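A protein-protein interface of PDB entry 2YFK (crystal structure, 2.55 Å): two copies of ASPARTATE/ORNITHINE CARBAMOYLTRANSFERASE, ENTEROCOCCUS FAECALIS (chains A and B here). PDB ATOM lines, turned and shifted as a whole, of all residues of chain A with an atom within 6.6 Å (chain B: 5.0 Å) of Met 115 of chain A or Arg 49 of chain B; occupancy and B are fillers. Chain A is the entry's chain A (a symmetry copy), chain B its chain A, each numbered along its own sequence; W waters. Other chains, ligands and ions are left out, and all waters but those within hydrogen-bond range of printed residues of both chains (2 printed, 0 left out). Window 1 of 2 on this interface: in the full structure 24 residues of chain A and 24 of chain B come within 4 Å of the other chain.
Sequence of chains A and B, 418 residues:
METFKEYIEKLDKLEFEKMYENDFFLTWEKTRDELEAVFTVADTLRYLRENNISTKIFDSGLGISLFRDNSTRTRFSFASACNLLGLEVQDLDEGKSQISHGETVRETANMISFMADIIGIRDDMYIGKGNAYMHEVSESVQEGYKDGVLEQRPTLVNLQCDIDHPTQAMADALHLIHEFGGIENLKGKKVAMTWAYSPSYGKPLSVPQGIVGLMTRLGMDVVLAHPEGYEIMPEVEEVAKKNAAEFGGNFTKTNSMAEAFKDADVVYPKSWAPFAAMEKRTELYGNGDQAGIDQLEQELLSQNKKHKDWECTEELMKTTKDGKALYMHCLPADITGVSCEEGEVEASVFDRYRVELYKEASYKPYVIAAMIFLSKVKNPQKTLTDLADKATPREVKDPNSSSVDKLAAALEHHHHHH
The backbone NH (N) of Arg 394 of chain B sits close to the side-chain amide oxygen (OD1) of Asn 52 of chain B. N of Leu 62 of chain A is in hydrogen-bond range of O of Met 115 of chain A. O of Leu 62 of chain A lies within hydrogen-bond range of N of Asp 117 of chain A (2.9 Å). O of Ser 113 of chain A lies within hydrogen-bond range of NE2 of Gln 152 of chain A, at 3.0 Å. The side-chain amide nitrogen (NE2) of Gln 152 of chain A is in hydrogen-bond range of the backbone carbonyl oxygen (O) of Phe 114 of chain A (3.2 Å). O of Ala 116 of chain A lies within hydrogen-bond range of NE2 of Gln 152 of chain A (3.3 Å).
Gly 61 of chain A touches Arg 394 of chain B (CA to NH2, 3.8 Å). Ser 80 of chain B touches Leu 62 of chain A (OG to CD1, 3.6 Å). Arg 49 of chain B touches Phe 114 of chain A. Met 115 of chain A touches Arg 49 of chain B. OG of Ser 80 of chain B touches CB of Met 115 of chain A, 3.7 Å away. Met 115 of chain A touches Pro 365 of chain B. CE of Met 115 of chain A touches CZ of Tyr 366 of chain B, at 3.97 Å.
NH1 of Arg 46 of chain B is in salt-bridge range of OE2 of Glu 151 of chain A. OE1 of Glu 151 of chain A lies within salt-bridge range of NH1 of Arg 49 of chain B (2.8 Å). The guanidinium group (NH1) of Arg 49 of chain B is in hydrogen-bond range of the side-chain amide oxygen (OE1) of Gln 152 of chain A, at 2.9 Å. The side-chain hydroxyl of Tyr 366 of chain B is in hydrogen-bond range of the side-chain carboxylate of Glu 151 of chain A (2.4 Å). The guanidinium group (NH2) of Arg 394 of chain B is in hydrogen-bond range of the backbone carbonyl oxygen (O) of Ser 60 of chain A (2.9 Å). The guanidinium group of Arg 394 of chain B lies within salt-bridge range of the side-chain carboxylate of Asp 117 of chain A.
Printed residues of chain B within 4 Å of Gly 61 of chain A: Arg 394 (3.8 Å). Met 115 of chain A touches just these residues of chain B: Arg 49 (3.5 Å), Ser 80 (3.7 Å), Pro 365 (3.6 Å) and Tyr 366 (3.97 Å). Arg 49 of chain B touches just these residues of chain A: Phe 114, Met 115, Glu 151 and Gln 152. Glu 50 of chain B touches none of the printed residues of chain A. Printed residues of chain A within 4 Å of Arg 394 of chain B: Ser 60, Gly 61 and Asp 117. The nearest residue of chain B that does not touch Met 115 of chain A is Leu 84 of chain B (4.2 Å).
Water W1 lies within hydrogen-bond range of OG of Ser 60 of chain A and O of Leu 84 of chain B. Water W2 lies within hydrogen-bond range of O of Ser 80 of chain B (3.1 Å) and SD of Met 115 of chain A (3.6 Å).
No position is printed for both chains. Of the 13 pairs that touch across the chains among the printed residues, none has its exchanged pair printed and touching as well.
Hydrophobic or aromatic side chains of chain A that line the printed part of chain B: Leu 62 and Met 115. Among the printed residues, 13 pairs touch across the chains.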
ATOM      1  N   SER A  60     -11.411 -15.394  -9.266  1.00  0.00           N
ATOM      2  CA  SER A  60     -11.667 -13.977  -9.569  1.00  0.00           C
ATOM      3  C   SER A  60     -10.778 -13.544 -10.734  1.00  0.00           C
ATOM      4  O   SER A  60      -9.872 -14.277 -11.127  1.00  0.00           O
ATOM      5  CB  SER A  60     -11.443 -13.080  -8.344  1.00  0.00           C
ATOM      6  OG  SER A  60     -10.073 -13.002  -7.978  1.00  0.00           O
ATOM      7  N   GLY A  61     -11.045 -12.366 -11.290  1.00  0.00           N
ATOM      8  CA  GLY A  61     -10.330 -11.881 -12.470  1.00  0.00           C
ATOM      9  C   GLY A  61     -11.270 -11.450 -13.583  1.00  0.00           C
ATOM     10  O   GLY A  61     -12.412 -11.922 -13.671  1.00  0.00           O
ATOM     11  N   LEU A  62     -10.778 -10.558 -14.444  1.00  0.00           N
ATOM     12  CA  LEU A  62     -11.588  -9.984 -15.503  1.00  0.00           C
ATOM     13  C   LEU A  62     -11.235 -10.517 -16.889  1.00  0.00           C
ATOM     14  O   LEU A  62     -10.108 -10.972 -17.140  1.00  0.00           O
ATOM     15  CB  LEU A  62     -11.444  -8.462 -15.506  1.00  0.00           C
ATOM     16  CG  LEU A  62     -11.699  -7.728 -14.187  1.00  0.00           C
ATOM     17  CD1 LEU A  62     -11.771  -6.230 -14.418  1.00  0.00           C
ATOM     18  CD2 LEU A  62     -12.966  -8.222 -13.533  1.00  0.00           C
ATOM     19  N   GLY A  63     -12.225 -10.462 -17.775  1.00  0.00           N
ATOM     20  CA  GLY A  63     -12.006 -10.606 -19.210  1.00  0.00           C
ATOM     21  C   GLY A  63     -12.450  -9.315 -19.879  1.00  0.00           C
ATOM     22  O   GLY A  63     -13.634  -8.991 -19.864  1.00  0.00           O
ATOM     23  N   ILE A  64     -11.506  -8.575 -20.452  1.00  0.00           N
ATOM     24  CA  ILE A  64     -11.809  -7.276 -21.043  1.00  0.00           C
ATOM     25  C   ILE A  64     -12.385  -7.474 -22.445  1.00  0.00           C
ATOM     26  O   ILE A  64     -11.734  -8.034 -23.323  1.00  0.00           O
ATOM     27  CB  ILE A  64     -10.560  -6.354 -21.131  1.00  0.00           C
ATOM     28  CG1 ILE A  64      -9.818  -6.275 -19.796  1.00  0.00           C
ATOM     29  CG2 ILE A  64     -10.957  -4.944 -21.560  1.00  0.00           C
ATOM     30  CD1 ILE A  64     -10.617  -5.678 -18.678  1.00  0.00           C
ATOM     31  N   LEU A  87     -14.586 -16.124 -15.251  1.00  0.00           N
ATOM     32  CA  LEU A  87     -14.161 -14.747 -15.461  1.00  0.00           C
ATOM     33  C   LEU A  87     -15.381 -13.848 -15.561  1.00  0.00           C
ATOM     34  O   LEU A  87     -16.444 -14.282 -16.006  1.00  0.00           O
ATOM     35  CB  LEU A  87     -13.324 -14.622 -16.737  1.00  0.00           C
ATOM     36  CG  LEU A  87     -11.950 -15.281 -16.688  1.00  0.00           C
ATOM     37  CD1 LEU A  87     -11.311 -15.310 -18.056  1.00  0.00           C
ATOM     38  CD2 LEU A  87     -11.059 -14.551 -15.693  1.00  0.00           C
ATOM     39  N   MET A 111      -3.457  -0.085 -18.410  1.00  0.00           N
ATOM     40  CA  MET A 111      -4.381   0.443 -17.398  1.00  0.00           C
ATOM     41  C   MET A 111      -5.603  -0.444 -17.162  1.00  0.00           C
ATOM     42  O   MET A 111      -6.111  -0.504 -16.040  1.00  0.00           O
ATOM     43  CB  MET A 111      -4.834   1.863 -17.759  1.00  0.00           C
ATOM     44  CG  MET A 111      -3.717   2.910 -17.765  1.00  0.00           C
ATOM     45  SD  MET A 111      -2.711   2.949 -16.266  1.00  0.00           S
ATOM     46  CE  MET A 111      -3.966   3.468 -15.097  1.00  0.00           C
ATOM     47  N   ILE A 112      -6.059  -1.133 -18.208  1.00  0.00           N
ATOM     48  CA  ILE A 112      -7.199  -2.054 -18.109  1.00  0.00           C
ATOM     49  C   ILE A 112      -6.814  -3.475 -17.658  1.00  0.00           C
ATOM     50  O   ILE A 112      -7.690  -4.268 -17.296  1.00  0.00           O
ATOM     51  CB  ILE A 112      -7.981  -2.165 -19.460  1.00  0.00           C
ATOM     52  CG1 ILE A 112      -7.165  -2.922 -20.518  1.00  0.00           C
ATOM     53  CG2 ILE A 112      -8.376  -0.794 -19.971  1.00  0.00           C
ATOM     54  CD1 ILE A 112      -7.611  -2.662 -21.961  1.00  0.00           C
ATOM     55  N   SER A 113      -5.519  -3.786 -17.663  1.00  0.00           N
ATOM     56  CA  SER A 113      -5.057  -5.167 -17.509  1.00  0.00           C
ATOM     57  C   SER A 113      -4.678  -5.609 -16.090  1.00  0.00           C
ATOM     58  O   SER A 113      -4.478  -6.805 -15.857  1.00  0.00           O
ATOM     59  CB  SER A 113      -3.867  -5.422 -18.443  1.00  0.00           C
ATOM     60  OG  SER A 113      -4.282  -5.436 -19.801  1.00  0.00           O
ATOM     61  N   PHE A 114      -4.598  -4.676 -15.143  1.00  0.00           N
ATOM     62  CA  PHE A 114      -4.066  -4.986 -13.808  1.00  0.00           C
ATOM     63  C   PHE A 114      -4.659  -6.253 -13.205  1.00  0.00           C
ATOM     64  O   PHE A 114      -3.946  -7.034 -12.578  1.00  0.00           O
ATOM     65  CB  PHE A 114      -4.258  -3.817 -12.837  1.00  0.00           C
ATOM     66  CG  PHE A 114      -3.432  -2.607 -13.168  1.00  0.00           C
ATOM     67  CD1 PHE A 114      -2.057  -2.712 -13.340  1.00  0.00           C
ATOM     68  CD2 PHE A 114      -4.022  -1.358 -13.289  1.00  0.00           C
ATOM     69  CE1 PHE A 114      -1.290  -1.595 -13.645  1.00  0.00           C
ATOM     70  CE2 PHE A 114      -3.261  -0.238 -13.595  1.00  0.00           C
ATOM     71  CZ  PHE A 114      -1.891  -0.359 -13.774  1.00  0.00           C
ATOM     72  N   MET A 115      -5.959  -6.454 -13.394  1.00  0.00           N
ATOM     73  CA  MET A 115      -6.606  -7.676 -12.935  1.00  0.00           C
ATOM     74  C   MET A 115      -7.414  -8.322 -14.052  1.00  0.00           C
ATOM     75  O   MET A 115      -8.503  -8.843 -13.827  1.00  0.00           O
ATOM     76  CB  MET A 115      -7.483  -7.372 -11.728  1.00  0.00           C
ATOM     77  CG  MET A 115      -6.722  -6.700 -10.611  1.00  0.00           C
ATOM     78  SD  MET A 115      -7.661  -6.671  -9.094  1.00  0.00           S
ATOM     79  CE  MET A 115      -6.546  -5.756  -8.021  1.00  0.00           C
ATOM     80  N   ALA A 116      -6.856  -8.300 -15.258  1.00  0.00           N
ATOM     81  CA  ALA A 116      -7.474  -8.913 -16.422  1.00  0.00           C
ATOM     82  C   ALA A 116      -6.626 -10.100 -16.839  1.00  0.00           C
ATOM     83  O   ALA A 116      -5.400  -9.992 -16.915  1.00  0.00           O
ATOM     84  CB  ALA A 116      -7.569  -7.903 -17.561  1.00  0.00           C
ATOM     85  N   ASP A 117      -7.267 -11.235 -17.095  1.00  0.00           N
ATOM     86  CA  ASP A 117      -6.554 -12.410 -17.605  1.00  0.00           C
ATOM     87  C   ASP A 117      -6.699 -12.548 -19.110  1.00  0.00           C
ATOM     88  O   ASP A 117      -5.807 -13.074 -19.773  1.00  0.00           O
ATOM     89  CB  ASP A 117      -7.052 -13.666 -16.908  1.00  0.00           C
ATOM     90  CG  ASP A 117      -6.770 -13.646 -15.422  1.00  0.00           C
ATOM     91  OD1 ASP A 117      -5.593 -13.481 -15.027  1.00  0.00           O
ATOM     92  OD2 ASP A 117      -7.726 -13.788 -14.638  1.00  0.00           O
ATOM     93  N   GLU A 151       0.856  -8.156 -12.943  1.00  0.00           N
ATOM     94  CA  GLU A 151       1.089  -9.429 -12.236  1.00  0.00           C
ATOM     95  C   GLU A 151       0.972 -10.643 -13.154  1.00  0.00           C
ATOM     96  O   GLU A 151       1.485 -11.712 -12.836  1.00  0.00           O
ATOM     97  CB  GLU A 151       0.106  -9.590 -11.066  1.00  0.00           C
ATOM     98  CG  GLU A 151       0.310  -8.573  -9.964  1.00  0.00           C
ATOM     99  CD  GLU A 151      -0.831  -8.538  -8.977  1.00  0.00           C
ATOM    100  OE1 GLU A 151      -1.593  -9.501  -8.845  1.00  0.00           O
ATOM    101  OE2 GLU A 151      -0.956  -7.424  -8.274  1.00  0.00           O
ATOM    102  N   GLN A 152       0.283 -10.477 -14.281  1.00  0.00           N
ATOM    103  CA  GLN A 152       0.124 -11.552 -15.259  1.00  0.00           C
ATOM    104  C   GLN A 152       0.214 -10.998 -16.677  1.00  0.00           C
ATOM    105  O   GLN A 152       0.332  -9.790 -16.878  1.00  0.00           O
ATOM    106  CB  GLN A 152      -1.199 -12.304 -15.050  1.00  0.00           C
ATOM    107  CG  GLN A 152      -2.463 -11.483 -15.313  1.00  0.00           C
ATOM    108  CD  GLN A 152      -2.738 -10.430 -14.257  1.00  0.00           C
ATOM    109  OE1 GLN A 152      -2.606 -10.681 -13.059  1.00  0.00           O
ATOM    110  NE2 GLN A 152      -3.133  -9.242 -14.701  1.00  0.00           N
ATOM    111  N   LEU B  45      -3.257  -7.731   0.343  1.00  0.00           N
ATOM    112  CA  LEU B  45      -4.068  -8.272  -0.758  1.00  0.00           C
ATOM    113  C   LEU B  45      -3.221  -8.507  -2.018  1.00  0.00           C
ATOM    114  O   LEU B  45      -3.397  -9.507  -2.719  1.00  0.00           O
ATOM    115  CB  LEU B  45      -5.241  -7.339  -1.078  1.00  0.00           C
ATOM    116  CG  LEU B  45      -6.290  -7.123   0.023  1.00  0.00           C
ATOM    117  CD1 LEU B  45      -7.184  -5.953  -0.319  1.00  0.00           C
ATOM    118  CD2 LEU B  45      -7.126  -8.363   0.258  1.00  0.00           C
ATOM    119  N   ARG B  46      -2.298  -7.589  -2.293  1.00  0.00           N
ATOM    120  CA  ARG B  46      -1.331  -7.776  -3.380  1.00  0.00           C
ATOM    121  C   ARG B  46      -0.483  -9.023  -3.136  1.00  0.00           C
ATOM    122  O   ARG B  46      -0.343  -9.873  -4.023  1.00  0.00           O
ATOM    123  CB  ARG B  46      -0.432  -6.546  -3.520  1.00  0.00           C
ATOM    124  CG  ARG B  46       0.486  -6.572  -4.737  1.00  0.00           C
ATOM    125  CD  ARG B  46       1.492  -5.426  -4.717  1.00  0.00           C
ATOM    126  NE  ARG B  46       0.914  -4.157  -5.159  1.00  0.00           N
ATOM    127  CZ  ARG B  46       0.861  -3.730  -6.426  1.00  0.00           C
ATOM    128  NH1 ARG B  46       1.344  -4.467  -7.425  1.00  0.00           N
ATOM    129  NH2 ARG B  46       0.320  -2.545  -6.702  1.00  0.00           N
ATOM    130  N   TYR B  47       0.070  -9.137  -1.930  1.00  0.00           N
ATOM    131  CA  TYR B  47       0.875 -10.299  -1.575  1.00  0.00           C
ATOM    132  C   TYR B  47       0.119 -11.594  -1.834  1.00  0.00           C
ATOM    133  O   TYR B  47       0.657 -12.516  -2.447  1.00  0.00           O
ATOM    134  CB  TYR B  47       1.321 -10.245  -0.109  1.00  0.00           C
ATOM    135  CG  TYR B  47       1.943 -11.538   0.365  1.00  0.00           C
ATOM    136  CD1 TYR B  47       3.270 -11.844   0.076  1.00  0.00           C
ATOM    137  CD2 TYR B  47       1.201 -12.462   1.093  1.00  0.00           C
ATOM    138  CE1 TYR B  47       3.837 -13.037   0.505  1.00  0.00           C
ATOM    139  CE2 TYR B  47       1.760 -13.652   1.528  1.00  0.00           C
ATOM    140  CZ  TYR B  47       3.072 -13.935   1.233  1.00  0.00           C
ATOM    141  OH  TYR B  47       3.612 -15.123   1.670  1.00  0.00           O
ATOM    142  N   LEU B  48      -1.127 -11.656  -1.375  1.00  0.00           N
ATOM    143  CA  LEU B  48      -1.930 -12.861  -1.538  1.00  0.00           C
ATOM    144  C   LEU B  48      -2.196 -13.177  -3.016  1.00  0.00           C
ATOM    145  O   LEU B  48      -1.958 -14.296  -3.459  1.00  0.00           O
ATOM    146  CB  LEU B  48      -3.228 -12.764  -0.731  1.00  0.00           C
ATOM    147  CG  LEU B  48      -3.011 -12.730   0.795  1.00  0.00           C
ATOM    148  CD1 LEU B  48      -4.309 -12.466   1.550  1.00  0.00           C
ATOM    149  CD2 LEU B  48      -2.366 -14.021   1.278  1.00  0.00           C
ATOM    150  N   ARG B  49      -2.644 -12.192  -3.784  1.00  0.00           N
ATOM    151  CA  ARG B  49      -2.880 -12.401  -5.216  1.00  0.00           C
ATOM    152  C   ARG B  49      -1.589 -12.751  -5.964  1.00  0.00           C
ATOM    153  O   ARG B  49      -1.602 -13.622  -6.831  1.00  0.00           O
ATOM    154  CB  ARG B  49      -3.542 -11.183  -5.853  1.00  0.00           C
ATOM    155  CG  ARG B  49      -4.120 -11.443  -7.236  1.00  0.00           C
ATOM    156  CD  ARG B  49      -4.828 -10.203  -7.750  1.00  0.00           C
ATOM    157  NE  ARG B  49      -5.578 -10.431  -8.984  1.00  0.00           N
ATOM    158  CZ  ARG B  49      -5.060 -10.424 -10.211  1.00  0.00           C
ATOM    159  NH1 ARG B  49      -3.760 -10.223 -10.403  1.00  0.00           N
ATOM    160  NH2 ARG B  49      -5.853 -10.633 -11.257  1.00  0.00           N
ATOM    161  N   GLU B  50      -0.479 -12.091  -5.630  1.00  0.00           N
ATOM    162  CA  GLU B  50       0.823 -12.456  -6.228  1.00  0.00           C
ATOM    163  C   GLU B  50       1.156 -13.933  -6.000  1.00  0.00           C
ATOM    164  O   GLU B  50       1.758 -14.571  -6.857  1.00  0.00           O
ATOM    165  CB  GLU B  50       1.964 -11.554  -5.725  1.00  0.00           C
ATOM    166  CG  GLU B  50       2.129 -10.254  -6.535  1.00  0.00           C
ATOM    167  CD  GLU B  50       3.012  -9.200  -5.850  1.00  0.00           C
ATOM    168  OE1 GLU B  50       3.744  -9.535  -4.887  1.00  0.00           O
ATOM    169  OE2 GLU B  50       2.976  -8.026  -6.284  1.00  0.00           O
ATOM    170  N   ASN B  51       0.730 -14.478  -4.863  1.00  0.00           N
ATOM    171  CA  ASN B  51       0.918 -15.901  -4.555  1.00  0.00           C
ATOM    172  C   ASN B  51      -0.282 -16.782  -4.891  1.00  0.00           C
ATOM    173  O   ASN B  51      -0.465 -17.843  -4.291  1.00  0.00           O
ATOM    174  CB  ASN B  51       1.270 -16.058  -3.079  1.00  0.00           C
ATOM    175  CG  ASN B  51       2.659 -15.575  -2.768  1.00  0.00           C
ATOM    176  OD1 ASN B  51       2.839 -14.528  -2.153  1.00  0.00           O
ATOM    177  ND2 ASN B  51       3.658 -16.332  -3.211  1.00  0.00           N
ATOM    178  N   ASN B  52      -1.085 -16.344  -5.855  1.00  0.00           N
ATOM    179  CA  ASN B  52      -2.238 -17.099  -6.331  1.00  0.00           C
ATOM    180  C   ASN B  52      -3.274 -17.446  -5.255  1.00  0.00           C
ATOM    181  O   ASN B  52      -3.905 -18.494  -5.328  1.00  0.00           O
ATOM    182  CB  ASN B  52      -1.770 -18.377  -7.044  1.00  0.00           C
ATOM    183  CG  ASN B  52      -2.848 -18.983  -7.929  1.00  0.00           C
ATOM    184  OD1 ASN B  52      -3.734 -18.285  -8.414  1.00  0.00           O
ATOM    185  ND2 ASN B  52      -2.781 -20.284  -8.130  1.00  0.00           N
ATOM    186  N   ILE B  53      -3.468 -16.567  -4.272  1.00  0.00           N
ATOM    187  CA  ILE B  53      -4.439 -16.824  -3.201  1.00  0.00           C
ATOM    188  C   ILE B  53      -5.657 -15.904  -3.287  1.00  0.00           C
ATOM    189  O   ILE B  53      -5.551 -14.699  -3.047  1.00  0.00           O
ATOM    190  CB  ILE B  53      -3.810 -16.677  -1.803  1.00  0.00           C
ATOM    191  CG1 ILE B  53      -2.764 -17.765  -1.572  1.00  0.00           C
ATOM    192  CG2 ILE B  53      -4.889 -16.778  -0.729  1.00  0.00           C
ATOM    193  CD1 ILE B  53      -1.891 -17.525  -0.368  1.00  0.00           C
ATOM    194  N   SER B  80     -12.571  -3.837 -10.762  1.00  0.00           N
ATOM    195  CA  SER B  80     -11.510  -4.755 -10.336  1.00  0.00           C
ATOM    196  C   SER B  80     -11.546  -5.051  -8.840  1.00  0.00           C
ATOM    197  O   SER B  80     -11.475  -6.210  -8.434  1.00  0.00           O
ATOM    198  CB  SER B  80     -10.136  -4.192 -10.685  1.00  0.00           C
ATOM    199  OG  SER B  80      -9.791  -4.492 -12.023  1.00  0.00           O
ATOM    200  N   ALA B  81     -11.633  -3.998  -8.027  1.00  0.00           N
ATOM    201  CA  ALA B  81     -11.632  -4.135  -6.569  1.00  0.00           C
ATOM    202  C   ALA B  81     -12.821  -4.970  -6.093  1.00  0.00           C
ATOM    203  O   ALA B  81     -12.668  -5.896  -5.295  1.00  0.00           O
ATOM    204  CB  ALA B  81     -11.645  -2.756  -5.907  1.00  0.00           C
ATOM    205  N   LEU B  84     -12.400  -8.680  -7.023  1.00  0.00           N
ATOM    206  CA  LEU B  84     -11.362  -9.289  -6.188  1.00  0.00           C
ATOM    207  C   LEU B  84     -11.922  -9.803  -4.868  1.00  0.00           C
ATOM    208  O   LEU B  84     -11.497 -10.849  -4.379  1.00  0.00           O
ATOM    209  CB  LEU B  84     -10.248  -8.275  -5.895  1.00  0.00           C
ATOM    210  CG  LEU B  84      -9.003  -8.789  -5.168  1.00  0.00           C
ATOM    211  CD1 LEU B  84      -8.163  -9.654  -6.094  1.00  0.00           C
ATOM    212  CD2 LEU B  84      -8.187  -7.631  -4.627  1.00  0.00           C
ATOM    213  N   PRO B 365      -6.393  -0.080  -7.725  1.00  0.00           N
ATOM    214  CA  PRO B 365      -7.317  -1.191  -7.468  1.00  0.00           C
ATOM    215  C   PRO B 365      -7.187  -1.768  -6.052  1.00  0.00           C
ATOM    216  O   PRO B 365      -8.194  -2.084  -5.406  1.00  0.00           O
ATOM    217  CB  PRO B 365      -6.903  -2.243  -8.501  1.00  0.00           C
ATOM    218  CG  PRO B 365      -6.173  -1.515  -9.549  1.00  0.00           C
ATOM    219  CD  PRO B 365      -5.544  -0.330  -8.902  1.00  0.00           C
ATOM    220  N   TYR B 366      -5.954  -1.910  -5.579  1.00  0.00           N
ATOM    221  CA  TYR B 366      -5.709  -2.432  -4.234  1.00  0.00           C
ATOM    222  C   TYR B 366      -6.121  -1.448  -3.129  1.00  0.00           C
ATOM    223  O   TYR B 366      -6.556  -1.864  -2.054  1.00  0.00           O
ATOM    224  CB  TYR B 366      -4.239  -2.818  -4.067  1.00  0.00           C
ATOM    225  CG  TYR B 366      -3.862  -4.095  -4.782  1.00  0.00           C
ATOM    226  CD1 TYR B 366      -4.354  -5.320  -4.355  1.00  0.00           C
ATOM    227  CD2 TYR B 366      -2.999  -4.080  -5.872  1.00  0.00           C
ATOM    228  CE1 TYR B 366      -4.008  -6.491  -4.995  1.00  0.00           C
ATOM    229  CE2 TYR B 366      -2.646  -5.251  -6.520  1.00  0.00           C
ATOM    230  CZ  TYR B 366      -3.153  -6.453  -6.079  1.00  0.00           C
ATOM    231  OH  TYR B 366      -2.802  -7.624  -6.710  1.00  0.00           O
ATOM    232  N   ARG B 394      -6.800 -18.673  -7.075  1.00  0.00           N
ATOM    233  CA  ARG B 394      -7.574 -17.879  -8.021  1.00  0.00           C
ATOM    234  C   ARG B 394      -7.361 -18.379  -9.453  1.00  0.00           C
ATOM    235  O   ARG B 394      -8.274 -18.316 -10.270  1.00  0.00           O
ATOM    236  CB  ARG B 394      -7.293 -16.377  -7.884  1.00  0.00           C
ATOM    237  CG  ARG B 394      -5.948 -15.898  -8.380  1.00  0.00           C
ATOM    238  CD  ARG B 394      -6.013 -14.426  -8.734  1.00  0.00           C
ATOM    239  NE  ARG B 394      -6.804 -14.235  -9.943  1.00  0.00           N
ATOM    240  CZ  ARG B 394      -6.326 -14.136 -11.185  1.00  0.00           C
ATOM    241  NH1 ARG B 394      -5.024 -14.172 -11.443  1.00  0.00           N
ATOM    242  NH2 ARG B 394      -7.181 -13.984 -12.189  1.00  0.00           N
HETATM  243  O   HOH W   1      -9.677 -12.843  -5.307  1.00  0.00           O
HETATM  244  O   HOH W   2     -10.538  -8.629 -10.045  1.00  0.00           O
